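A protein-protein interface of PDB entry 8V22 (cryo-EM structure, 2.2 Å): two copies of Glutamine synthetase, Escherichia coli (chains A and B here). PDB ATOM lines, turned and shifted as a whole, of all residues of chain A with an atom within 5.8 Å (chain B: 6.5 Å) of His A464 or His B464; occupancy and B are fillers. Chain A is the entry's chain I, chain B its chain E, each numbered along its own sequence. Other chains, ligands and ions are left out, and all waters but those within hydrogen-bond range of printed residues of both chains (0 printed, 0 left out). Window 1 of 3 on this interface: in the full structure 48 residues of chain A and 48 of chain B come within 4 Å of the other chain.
Val A155 touches Phe B468, and with the chains exchanged Phe A468 touches Val B155.
Asn A323 touches Glu B467, and with the chains exchanged Glu A467 touches Asn B323.
Lys A326 touches Pro B463, and with the chains exchanged Pro A463 touches Lys B326.
Val A459 touches Glu B467, and with the chains exchanged Glu A467 touches Val B459.
13 positions are printed for both chains.
Of the 32 pairs that touch across the chains among the printed residues, 27 have their exchanged pair printed and touching as well.
The backbone NH of Val B155 is in hydrogen-bond range of the backbone carbonyl oxygen of Ser A153 (2.9 Å).
The side-chain carboxylate of Glu A467 lies within hydrogen-bond range of the side-chain hydroxyl of Thr B322 (2.8 Å).
The side-chain amino group (NZ) of Lys A326 lies within salt-bridge range of the side-chain carboxylate (OE2) of Glu B467 (2.6 Å).
A ring nitrogen (NE2) of His A464 is in hydrogen-bond range of the backbone carbonyl oxygen (O) of Pro B463, at 3.3 Å.
The backbone NH (N) of Val A155 sits at hydrogen-bond distance from the backbone carbonyl oxygen (O) of Ser B153 (2.9 Å).
A ring nitrogen (NE2) of His A464 is in hydrogen-bond range of the backbone carbonyl oxygen (O) of Thr B462 (2.9 Å).
The side-chain carboxylate (OE2) of Glu A467 is in salt-bridge range of the side-chain amino group (NZ) of Lys B326 (2.6 Å).
The side-chain amide nitrogen (ND2) of Asn A323 sits at hydrogen-bond distance from the side-chain carboxylate (OE1) of Glu B467 (2.8 Å).
O of Thr A462 sits at hydrogen-bond distance from NE2 of His B464.
O of Pro A463 sits at hydrogen-bond distance from NE2 of His B464.
OE1 of Glu A469 is in salt-bridge range of NH2 of Arg B458 (3.5 Å).
The side-chain carboxylate (OE1) of Glu A467 is in hydrogen-bond range of the side-chain amide nitrogen (ND2) of Asn B323.
Among the printed residues, merely in contact across the chains: Lys A326 with Thr B462 (3.0 Å), Thr A462 with Lys B326 (3.0 Å), Lys A326 with Arg B460 (3.3 Å), Val A466 with Thr B462 (3.4 Å), Thr A462 with Val B466 (3.4 Å), Val A466 with Arg B458 (3.5 Å), Pro A463 with Lys B326 (3.5 Å), Lys A326 with Pro B463 (3.5 Å), His A464 with His B464 (3.5 Å), Phe A468 with Val B155 (3.5 Å), Val A155 with Phe B468 (3.6 Å), Pro A463 with Lys B264 (3.6 Å), Val A466 with Val B459 (3.6 Å), Val A459 with Val B466 (3.6 Å), Pro A463 with Asn B323 (3.8 Å), Asn A323 with Pro B463 (3.9 Å), Glu A467 with Val B459 (3.9 Å), Pro A465 with Val B155 (3.9 Å), Val A459 with Glu B467 (3.9 Å) and Val A155 with Pro B465 (3.9 Å).
Hydrophobic or aromatic side chains of chain A within 4 Å of the printed part of chain B: Val A155, Val A459, Pro A463, His A464, Pro A465, Val A466 and Phe A468.
Printed residues of chain B that touch a printed residue of chain A: Ser B153, Val B155, Lys B264, Thr B322, Asn B323, Lys B326, Arg B458, Val B459, Arg B460, Thr B462, Pro B463, His B464, Pro B465, Val B466, Glu B467 and Phe B468.
Hydrophobic or aromatic side chains of chain B that line the printed part of chain A: Val B155, Val B459, Pro B463, His B464, Pro B465, Val B466 and Phe B468.
Of chain A, only Thr A462, Pro A463 and His A464 come within 4 Å of His B464.
Printed residues of chain B within 4 Å of Thr A462: Lys B326, His B464 and Val B466.
Of the printed residues of chain B, Glu A469 touches Arg B458 (3.5 Å).
Of the printed residues of chain A, Arg B460 touches Lys A326.
Of the printed residues of chain B, Asn A323 touches Pro B463 (3.9 Å) and Glu B467 (2.8 Å).
The nearest residue of chain A that does not touch His B464 is Val A459 (4.03 Å).
The side-chain hydroxyl (OG1) of Thr B462 lies within hydrogen-bond range of the backbone carbonyl oxygen (O) of Arg B458 (2.7 Å).
OE1 of Glu A467 lies within hydrogen-bond range of N of His A464.
ND1 of His A464 sits at hydrogen-bond distance from N of Val A466 (3.1 Å).
A ring nitrogen (ND1) of His B464 sits at hydrogen-bond distance from the backbone NH (N) of Val B466, 3.1 Å away.
The side-chain amide oxygen (OD1) of Asn B323 is in hydrogen-bond range of the backbone NH (N) of Lys B264 (2.6 Å).
The backbone NH of His B464 lies within hydrogen-bond range of the side-chain carboxylate of Glu B467 (3.0 Å).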
ATOM      1  N   SER A 153      19.020  11.285  -4.959  1.00  0.00           N
ATOM      2  CA  SER A 153      20.238  11.613  -5.686  1.00  0.00           C
ATOM      3  C   SER A 153      19.969  12.773  -6.630  1.00  0.00           C
ATOM      4  O   SER A 153      18.871  12.906  -7.167  1.00  0.00           O
ATOM      5  CB  SER A 153      20.751  10.408  -6.478  1.00  0.00           C
ATOM      6  OG  SER A 153      19.771   9.967  -7.400  1.00  0.00           O
ATOM      7  N   VAL A 155      21.942  15.745  -9.588  1.00  0.00           N
ATOM      8  CA  VAL A 155      22.998  16.425 -10.325  1.00  0.00           C
ATOM      9  C   VAL A 155      22.422  17.721 -10.873  1.00  0.00           C
ATOM     10  O   VAL A 155      21.298  17.744 -11.388  1.00  0.00           O
ATOM     11  CB  VAL A 155      23.571  15.571 -11.472  1.00  0.00           C
ATOM     12  CG1 VAL A 155      22.486  15.232 -12.474  1.00  0.00           C
ATOM     13  CG2 VAL A 155      24.715  16.313 -12.153  1.00  0.00           C
ATOM     14  N   ASN A 323      28.503   6.320 -18.683  1.00  0.00           N
ATOM     15  CA  ASN A 323      28.108   7.551 -19.345  1.00  0.00           C
ATOM     16  C   ASN A 323      28.495   7.543 -20.816  1.00  0.00           C
ATOM     17  O   ASN A 323      27.798   8.154 -21.633  1.00  0.00           O
ATOM     18  CB  ASN A 323      28.752   8.739 -18.629  1.00  0.00           C
ATOM     19  CG  ASN A 323      28.090  10.055 -18.962  1.00  0.00           C
ATOM     20  OD1 ASN A 323      28.656  10.885 -19.669  1.00  0.00           O
ATOM     21  ND2 ASN A 323      26.888  10.261 -18.440  1.00  0.00           N
ATOM     22  N   LYS A 326      25.833   6.657 -23.212  1.00  0.00           N
ATOM     23  CA  LYS A 326      24.776   7.639 -23.380  1.00  0.00           C
ATOM     24  C   LYS A 326      25.059   8.616 -24.511  1.00  0.00           C
ATOM     25  O   LYS A 326      24.181   9.419 -24.843  1.00  0.00           O
ATOM     26  CB  LYS A 326      24.562   8.392 -22.067  1.00  0.00           C
ATOM     27  CG  LYS A 326      23.926   7.521 -21.009  1.00  0.00           C
ATOM     28  CD  LYS A 326      23.909   8.178 -19.659  1.00  0.00           C
ATOM     29  CE  LYS A 326      23.121   7.349 -18.665  1.00  0.00           C
ATOM     30  NZ  LYS A 326      23.667   5.975 -18.519  1.00  0.00           N
ATOM     31  N   VAL A 459      26.260   2.074 -10.829  1.00  0.00           N
ATOM     32  CA  VAL A 459      25.302   2.792 -11.665  1.00  0.00           C
ATOM     33  C   VAL A 459      24.071   1.938 -11.938  1.00  0.00           C
ATOM     34  O   VAL A 459      22.964   2.464 -12.099  1.00  0.00           O
ATOM     35  CB  VAL A 459      25.970   3.244 -12.975  1.00  0.00           C
ATOM     36  CG1 VAL A 459      24.945   3.849 -13.917  1.00  0.00           C
ATOM     37  CG2 VAL A 459      27.071   4.239 -12.690  1.00  0.00           C
ATOM     38  N   THR A 462      21.890   1.960  -8.546  1.00  0.00           N
ATOM     39  CA  THR A 462      21.307   3.175  -7.972  1.00  0.00           C
ATOM     40  C   THR A 462      20.071   3.610  -8.761  1.00  0.00           C
ATOM     41  O   THR A 462      20.142   3.729  -9.989  1.00  0.00           O
ATOM     42  CB  THR A 462      22.314   4.311  -7.939  1.00  0.00           C
ATOM     43  OG1 THR A 462      23.587   3.817  -7.507  1.00  0.00           O
ATOM     44  CG2 THR A 462      21.842   5.395  -6.990  1.00  0.00           C
ATOM     45  N   PRO A 463      18.935   3.860  -8.102  1.00  0.00           N
ATOM     46  CA  PRO A 463      17.730   4.282  -8.829  1.00  0.00           C
ATOM     47  C   PRO A 463      17.922   5.602  -9.559  1.00  0.00           C
ATOM     48  O   PRO A 463      18.814   6.392  -9.244  1.00  0.00           O
ATOM     49  CB  PRO A 463      16.678   4.414  -7.726  1.00  0.00           C
ATOM     50  CG  PRO A 463      17.137   3.531  -6.657  1.00  0.00           C
ATOM     51  CD  PRO A 463      18.630   3.573  -6.690  1.00  0.00           C
ATOM     52  N   HIS A 464      17.062   5.831 -10.549  1.00  0.00           N
ATOM     53  CA  HIS A 464      17.180   6.965 -11.452  1.00  0.00           C
ATOM     54  C   HIS A 464      16.027   7.955 -11.262  1.00  0.00           C
ATOM     55  O   HIS A 464      14.861   7.545 -11.140  1.00  0.00           O
ATOM     56  CB  HIS A 464      17.190   6.473 -12.899  1.00  0.00           C
ATOM     57  CG  HIS A 464      17.951   7.355 -13.835  1.00  0.00           C
ATOM     58  ND1 HIS A 464      17.671   8.694 -13.993  1.00  0.00           N
ATOM     59  CD2 HIS A 464      18.971   7.083 -14.681  1.00  0.00           C
ATOM     60  CE1 HIS A 464      18.494   9.212 -14.884  1.00  0.00           C
ATOM     61  NE2 HIS A 464      19.292   8.255 -15.320  1.00  0.00           N
ATOM     62  N   PRO A 465      16.302   9.263 -11.232  1.00  0.00           N
ATOM     63  CA  PRO A 465      15.192  10.231 -11.211  1.00  0.00           C
ATOM     64  C   PRO A 465      14.226  10.070 -12.369  1.00  0.00           C
ATOM     65  O   PRO A 465      13.018  10.283 -12.204  1.00  0.00           O
ATOM     66  CB  PRO A 465      15.915  11.581 -11.261  1.00  0.00           C
ATOM     67  CG  PRO A 465      17.234  11.322 -10.656  1.00  0.00           C
ATOM     68  CD  PRO A 465      17.601   9.913 -10.992  1.00  0.00           C
ATOM     69  N   VAL A 466      14.728   9.716 -13.551  1.00  0.00           N
ATOM     70  CA  VAL A 466      13.839   9.408 -14.663  1.00  0.00           C
ATOM     71  C   VAL A 466      12.987   8.192 -14.333  1.00  0.00           C
ATOM     72  O   VAL A 466      11.813   8.121 -14.718  1.00  0.00           O
ATOM     73  CB  VAL A 466      14.657   9.214 -15.953  1.00  0.00           C
ATOM     74  CG1 VAL A 466      13.808   8.611 -17.056  1.00  0.00           C
ATOM     75  CG2 VAL A 466      15.226  10.538 -16.408  1.00  0.00           C
ATOM     76  N   GLU A 467      13.546   7.225 -13.602  1.00  0.00           N
ATOM     77  CA  GLU A 467      12.730   6.101 -13.160  1.00  0.00           C
ATOM     78  C   GLU A 467      11.609   6.556 -12.243  1.00  0.00           C
ATOM     79  O   GLU A 467      10.490   6.043 -12.343  1.00  0.00           O
ATOM     80  CB  GLU A 467      13.581   5.046 -12.456  1.00  0.00           C
ATOM     81  CG  GLU A 467      14.420   4.230 -13.398  1.00  0.00           C
ATOM     82  CD  GLU A 467      15.290   3.230 -12.678  1.00  0.00           C
ATOM     83  OE1 GLU A 467      15.495   3.386 -11.457  1.00  0.00           O
ATOM     84  OE2 GLU A 467      15.750   2.272 -13.331  1.00  0.00           O
ATOM     85  N   PHE A 468      11.871   7.510 -11.350  1.00  0.00           N
ATOM     86  CA  PHE A 468      10.759   8.032 -10.559  1.00  0.00           C
ATOM     87  C   PHE A 468       9.733   8.726 -11.442  1.00  0.00           C
ATOM     88  O   PHE A 468       8.530   8.460 -11.328  1.00  0.00           O
ATOM     89  CB  PHE A 468      11.259   8.983  -9.475  1.00  0.00           C
ATOM     90  CG  PHE A 468      12.002   8.302  -8.367  1.00  0.00           C
ATOM     91  CD1 PHE A 468      13.288   7.840  -8.550  1.00  0.00           C
ATOM     92  CD2 PHE A 468      11.409   8.140  -7.129  1.00  0.00           C
ATOM     93  CE1 PHE A 468      13.961   7.220  -7.527  1.00  0.00           C
ATOM     94  CE2 PHE A 468      12.079   7.522  -6.105  1.00  0.00           C
ATOM     95  CZ  PHE A 468      13.356   7.064  -6.304  1.00  0.00           C
ATOM     96  N   GLU A 469      10.195   9.571 -12.366  1.00  0.00           N
ATOM     97  CA  GLU A 469       9.272  10.283 -13.246  1.00  0.00           C
ATOM     98  C   GLU A 469       8.388   9.319 -14.017  1.00  0.00           C
ATOM     99  O   GLU A 469       7.235   9.637 -14.322  1.00  0.00           O
ATOM    100  CB  GLU A 469      10.044  11.161 -14.231  1.00  0.00           C
ATOM    101  CG  GLU A 469      10.736  12.352 -13.611  1.00  0.00           C
ATOM    102  CD  GLU A 469      11.483  13.176 -14.636  1.00  0.00           C
ATOM    103  OE1 GLU A 469      11.574  12.734 -15.800  1.00  0.00           O
ATOM    104  OE2 GLU A 469      11.989  14.260 -14.279  1.00  0.00           O
ATOM    105  N   SER B 153      19.237  16.488 -13.128  1.00  0.00           N
ATOM    106  CA  SER B 153      18.101  15.682 -12.709  1.00  0.00           C
ATOM    107  C   SER B 153      18.219  15.387 -11.224  1.00  0.00           C
ATOM    108  O   SER B 153      19.322  15.230 -10.701  1.00  0.00           O
ATOM    109  CB  SER B 153      18.026  14.371 -13.494  1.00  0.00           C
ATOM    110  OG  SER B 153      19.206  13.610 -13.315  1.00  0.00           O
ATOM    111  N   VAL B 155      16.094  13.459  -7.604  1.00  0.00           N
ATOM    112  CA  VAL B 155      15.039  12.819  -6.831  1.00  0.00           C
ATOM    113  C   VAL B 155      15.379  12.981  -5.358  1.00  0.00           C
ATOM    114  O   VAL B 155      16.534  12.806  -4.955  1.00  0.00           O
ATOM    115  CB  VAL B 155      14.866  11.329  -7.182  1.00  0.00           C
ATOM    116  CG1 VAL B 155      16.144  10.563  -6.903  1.00  0.00           C
ATOM    117  CG2 VAL B 155      13.712  10.737  -6.386  1.00  0.00           C
ATOM    118  N   LYS B 264      11.859  -0.328  -6.349  1.00  0.00           N
ATOM    119  CA  LYS B 264      13.076   0.092  -5.652  1.00  0.00           C
ATOM    120  C   LYS B 264      13.157   1.609  -5.633  1.00  0.00           C
ATOM    121  O   LYS B 264      13.815   2.228  -6.475  1.00  0.00           O
ATOM    122  CB  LYS B 264      14.315  -0.506  -6.315  1.00  0.00           C
ATOM    123  CG  LYS B 264      15.573  -0.425  -5.476  1.00  0.00           C
ATOM    124  CD  LYS B 264      15.622  -1.530  -4.439  1.00  0.00           C
ATOM    125  CE  LYS B 264      16.970  -1.576  -3.750  1.00  0.00           C
ATOM    126  NZ  LYS B 264      17.077  -2.721  -2.812  1.00  0.00           N
ATOM    127  N   THR B 322      12.364  -0.551 -15.520  1.00  0.00           N
ATOM    128  CA  THR B 322      13.802  -0.578 -15.296  1.00  0.00           C
ATOM    129  C   THR B 322      14.101  -0.633 -13.807  1.00  0.00           C
ATOM    130  O   THR B 322      14.961  -1.404 -13.360  1.00  0.00           O
ATOM    131  CB  THR B 322      14.459   0.645 -15.936  1.00  0.00           C
ATOM    132  OG1 THR B 322      13.931   1.838 -15.348  1.00  0.00           O
ATOM    133  CG2 THR B 322      14.211   0.667 -17.431  1.00  0.00           C
ATOM    134  N   ASN B 323      13.350   0.130 -13.015  1.00  0.00           N
ATOM    135  CA  ASN B 323      13.539   0.120 -11.574  1.00  0.00           C
ATOM    136  C   ASN B 323      13.395  -1.283 -11.004  1.00  0.00           C
ATOM    137  O   ASN B 323      14.040  -1.599  -9.998  1.00  0.00           O
ATOM    138  CB  ASN B 323      12.532   1.070 -10.927  1.00  0.00           C
ATOM    139  CG  ASN B 323      12.908   1.447  -9.513  1.00  0.00           C
ATOM    140  OD1 ASN B 323      12.277   1.009  -8.552  1.00  0.00           O
ATOM    141  ND2 ASN B 323      13.940   2.271  -9.377  1.00  0.00           N
ATOM    142  N   LYS B 326      16.520  -3.121 -10.355  1.00  0.00           N
ATOM    143  CA  LYS B 326      17.325  -2.634  -9.250  1.00  0.00           C
ATOM    144  C   LYS B 326      16.989  -3.326  -7.937  1.00  0.00           C
ATOM    145  O   LYS B 326      17.692  -3.106  -6.945  1.00  0.00           O
ATOM    146  CB  LYS B 326      17.151  -1.121  -9.120  1.00  0.00           C
ATOM    147  CG  LYS B 326      17.806  -0.378 -10.264  1.00  0.00           C
ATOM    148  CD  LYS B 326      17.464   1.085 -10.273  1.00  0.00           C
ATOM    149  CE  LYS B 326      18.268   1.820 -11.328  1.00  0.00           C
ATOM    150  NZ  LYS B 326      18.046   1.272 -12.691  1.00  0.00           N
ATOM    151  N   ARG B 458      14.324   6.140 -22.496  1.00  0.00           N
ATOM    152  CA  ARG B 458      14.457   7.344 -21.677  1.00  0.00           C
ATOM    153  C   ARG B 458      15.472   7.127 -20.561  1.00  0.00           C
ATOM    154  O   ARG B 458      16.401   7.930 -20.379  1.00  0.00           O
ATOM    155  CB  ARG B 458      13.098   7.748 -21.099  1.00  0.00           C
ATOM    156  CG  ARG B 458      12.187   8.417 -22.110  1.00  0.00           C
ATOM    157  CD  ARG B 458      11.173   9.361 -21.473  1.00  0.00           C
ATOM    158  NE  ARG B 458      11.794  10.521 -20.843  1.00  0.00           N
ATOM    159  CZ  ARG B 458      11.737  10.812 -19.548  1.00  0.00           C
ATOM    160  NH1 ARG B 458      11.068  10.054 -18.693  1.00  0.00           N
ATOM    161  NH2 ARG B 458      12.355  11.900 -19.101  1.00  0.00           N
ATOM    162  N   VAL B 459      15.334   6.022 -19.826  1.00  0.00           N
ATOM    163  CA  VAL B 459      16.227   5.789 -18.693  1.00  0.00           C
ATOM    164  C   VAL B 459      17.646   5.508 -19.169  1.00  0.00           C
ATOM    165  O   VAL B 459      18.617   5.832 -18.475  1.00  0.00           O
ATOM    166  CB  VAL B 459      15.698   4.643 -17.813  1.00  0.00           C
ATOM    167  CG1 VAL B 459      16.705   4.293 -16.731  1.00  0.00           C
ATOM    168  CG2 VAL B 459      14.376   5.022 -17.190  1.00  0.00           C
ATOM    169  N   ARG B 460      17.795   4.902 -20.344  1.00  0.00           N
ATOM    170  CA  ARG B 460      19.115   4.587 -20.873  1.00  0.00           C
ATOM    171  C   ARG B 460      19.846   5.823 -21.369  1.00  0.00           C
ATOM    172  O   ARG B 460      21.075   5.894 -21.264  1.00  0.00           O
ATOM    173  CB  ARG B 460      18.982   3.580 -22.015  1.00  0.00           C
ATOM    174  CG  ARG B 460      20.290   2.991 -22.496  1.00  0.00           C
ATOM    175  CD  ARG B 460      20.041   1.745 -23.323  1.00  0.00           C
ATOM    176  NE  ARG B 460      18.971   1.943 -24.292  1.00  0.00           N
ATOM    177  CZ  ARG B 460      19.109   2.595 -25.439  1.00  0.00           C
ATOM    178  NH1 ARG B 460      20.263   3.135 -25.793  1.00  0.00           N
ATOM    179  NH2 ARG B 460      18.062   2.710 -26.249  1.00  0.00           N
ATOM    180  N   MET B 461      19.121   6.797 -21.912  1.00  0.00           N
ATOM    181  CA  MET B 461      19.735   7.998 -22.456  1.00  0.00           C
ATOM    182  C   MET B 461      19.841   9.141 -21.454  1.00  0.00           C
ATOM    183  O   MET B 461      20.535  10.119 -21.745  1.00  0.00           O
ATOM    184  CB  MET B 461      18.956   8.483 -23.680  1.00  0.00           C
ATOM    185  CG  MET B 461      18.733   7.429 -24.745  1.00  0.00           C
ATOM    186  SD  MET B 461      17.686   8.039 -26.074  1.00  0.00           S
ATOM    187  CE  MET B 461      18.094   6.893 -27.384  1.00  0.00           C
ATOM    188  N   THR B 462      19.184   9.057 -20.284  1.00  0.00           N
ATOM    189  CA  THR B 462      19.376  10.176 -19.357  1.00  0.00           C
ATOM    190  C   THR B 462      20.583   9.929 -18.452  1.00  0.00           C
ATOM    191  O   THR B 462      20.681   8.859 -17.841  1.00  0.00           O
ATOM    192  CB  THR B 462      18.141  10.408 -18.505  1.00  0.00           C
ATOM    193  OG1 THR B 462      16.965  10.303 -19.318  1.00  0.00           O
ATOM    194  CG2 THR B 462      18.196  11.785 -17.874  1.00  0.00           C
ATOM    195  N   PRO B 463      21.514  10.885 -18.337  1.00  0.00           N
ATOM    196  CA  PRO B 463      22.689  10.681 -17.478  1.00  0.00           C
ATOM    197  C   PRO B 463      22.322  10.508 -16.012  1.00  0.00           C
ATOM    198  O   PRO B 463      21.238  10.893 -15.566  1.00  0.00           O
ATOM    199  CB  PRO B 463      23.506  11.958 -17.689  1.00  0.00           C
ATOM    200  CG  PRO B 463      23.104  12.454 -19.002  1.00  0.00           C
ATOM    201  CD  PRO B 463      21.661  12.096 -19.161  1.00  0.00           C
ATOM    202  N   HIS B 464      23.254   9.923 -15.259  1.00  0.00           N
ATOM    203  CA  HIS B 464      23.016   9.525 -13.880  1.00  0.00           C
ATOM    204  C   HIS B 464      23.864  10.342 -12.901  1.00  0.00           C
ATOM    205  O   HIS B 464      25.061  10.569 -13.145  1.00  0.00           O
ATOM    206  CB  HIS B 464      23.340   8.042 -13.707  1.00  0.00           C
ATOM    207  CG  HIS B 464      22.548   7.368 -12.634  1.00  0.00           C
ATOM    208  ND1 HIS B 464      22.534   7.809 -11.329  1.00  0.00           N
ATOM    209  CD2 HIS B 464      21.762   6.268 -12.665  1.00  0.00           C
ATOM    210  CE1 HIS B 464      21.761   7.020 -10.608  1.00  0.00           C
ATOM    211  NE2 HIS B 464      21.282   6.074 -11.394  1.00  0.00           N
ATOM    212  N   PRO B 465      23.288  10.796 -11.781  1.00  0.00           N
ATOM    213  CA  PRO B 465      24.123  11.442 -10.753  1.00  0.00           C
ATOM    214  C   PRO B 465      25.257  10.569 -10.251  1.00  0.00           C
ATOM    215  O   PRO B 465      26.341  11.081  -9.944  1.00  0.00           O
ATOM    216  CB  PRO B 465      23.114  11.750  -9.640  1.00  0.00           C
ATOM    217  CG  PRO B 465      21.822  11.887 -10.332  1.00  0.00           C
ATOM    218  CD  PRO B 465      21.852  10.963 -11.505  1.00  0.00           C
ATOM    219  N   VAL B 466      25.038   9.259 -10.139  1.00  0.00           N
ATOM    220  CA  VAL B 466      26.135   8.361  -9.801  1.00  0.00           C
ATOM    221  C   VAL B 466      27.189   8.388 -10.896  1.00  0.00           C
ATOM    222  O   VAL B 466      28.392   8.300 -10.616  1.00  0.00           O
ATOM    223  CB  VAL B 466      25.601   6.938  -9.549  1.00  0.00           C
ATOM    224  CG1 VAL B 466      26.733   5.931  -9.488  1.00  0.00           C
ATOM    225  CG2 VAL B 466      24.814   6.904  -8.259  1.00  0.00           C
ATOM    226  N   GLU B 467      26.765   8.520 -12.154  1.00  0.00           N
ATOM    227  CA  GLU B 467      27.741   8.661 -13.227  1.00  0.00           C
ATOM    228  C   GLU B 467      28.576   9.918 -13.056  1.00  0.00           C
ATOM    229  O   GLU B 467      29.784   9.890 -13.304  1.00  0.00           O
ATOM    230  CB  GLU B 467      27.057   8.670 -14.592  1.00  0.00           C
ATOM    231  CG  GLU B 467      26.581   7.314 -15.037  1.00  0.00           C
ATOM    232  CD  GLU B 467      25.864   7.362 -16.362  1.00  0.00           C
ATOM    233  OE1 GLU B 467      25.445   8.462 -16.777  1.00  0.00           O
ATOM    234  OE2 GLU B 467      25.736   6.298 -17.001  1.00  0.00           O
ATOM    235  N   PHE B 468      27.968  11.028 -12.635  1.00  0.00           N
ATOM    236  CA  PHE B 468      28.794  12.197 -12.337  1.00  0.00           C
ATOM    237  C   PHE B 468      29.745  11.923 -11.180  1.00  0.00           C
ATOM    238  O   PHE B 468      30.945  12.207 -11.280  1.00  0.00           O
ATOM    239  CB  PHE B 468      27.925  13.414 -12.034  1.00  0.00           C
ATOM    240  CG  PHE B 468      27.212  13.962 -13.232  1.00  0.00           C
ATOM    241  CD1 PHE B 468      26.119  13.318 -13.768  1.00  0.00           C
ATOM    242  CD2 PHE B 468      27.641  15.137 -13.816  1.00  0.00           C
ATOM    243  CE1 PHE B 468      25.473  13.828 -14.867  1.00  0.00           C
ATOM    244  CE2 PHE B 468      27.000  15.651 -14.914  1.00  0.00           C
ATOM    245  CZ  PHE B 468      25.913  14.995 -15.440  1.00  0.00           C
ATOM    246  N   GLU B 469      29.241  11.319 -10.102  1.00  0.00           N
ATOM    247  CA  GLU B 469      30.090  11.034  -8.949  1.00  0.00           C
ATOM    248  C   GLU B 469      31.287  10.185  -9.341  1.00  0.00           C
ATOM    249  O   GLU B 469      32.364  10.313  -8.748  1.00  0.00           O
ATOM    250  CB  GLU B 469      29.295  10.313  -7.862  1.00  0.00           C
ATOM    251  CG  GLU B 469      28.252  11.161  -7.174  1.00  0.00           C
ATOM    252  CD  GLU B 469      27.499  10.393  -6.110  1.00  0.00           C
ATOM    253  OE1 GLU B 469      27.695   9.162  -6.016  1.00  0.00           O
ATOM    254  OE2 GLU B 469      26.703  11.011  -5.373  1.00  0.00           O
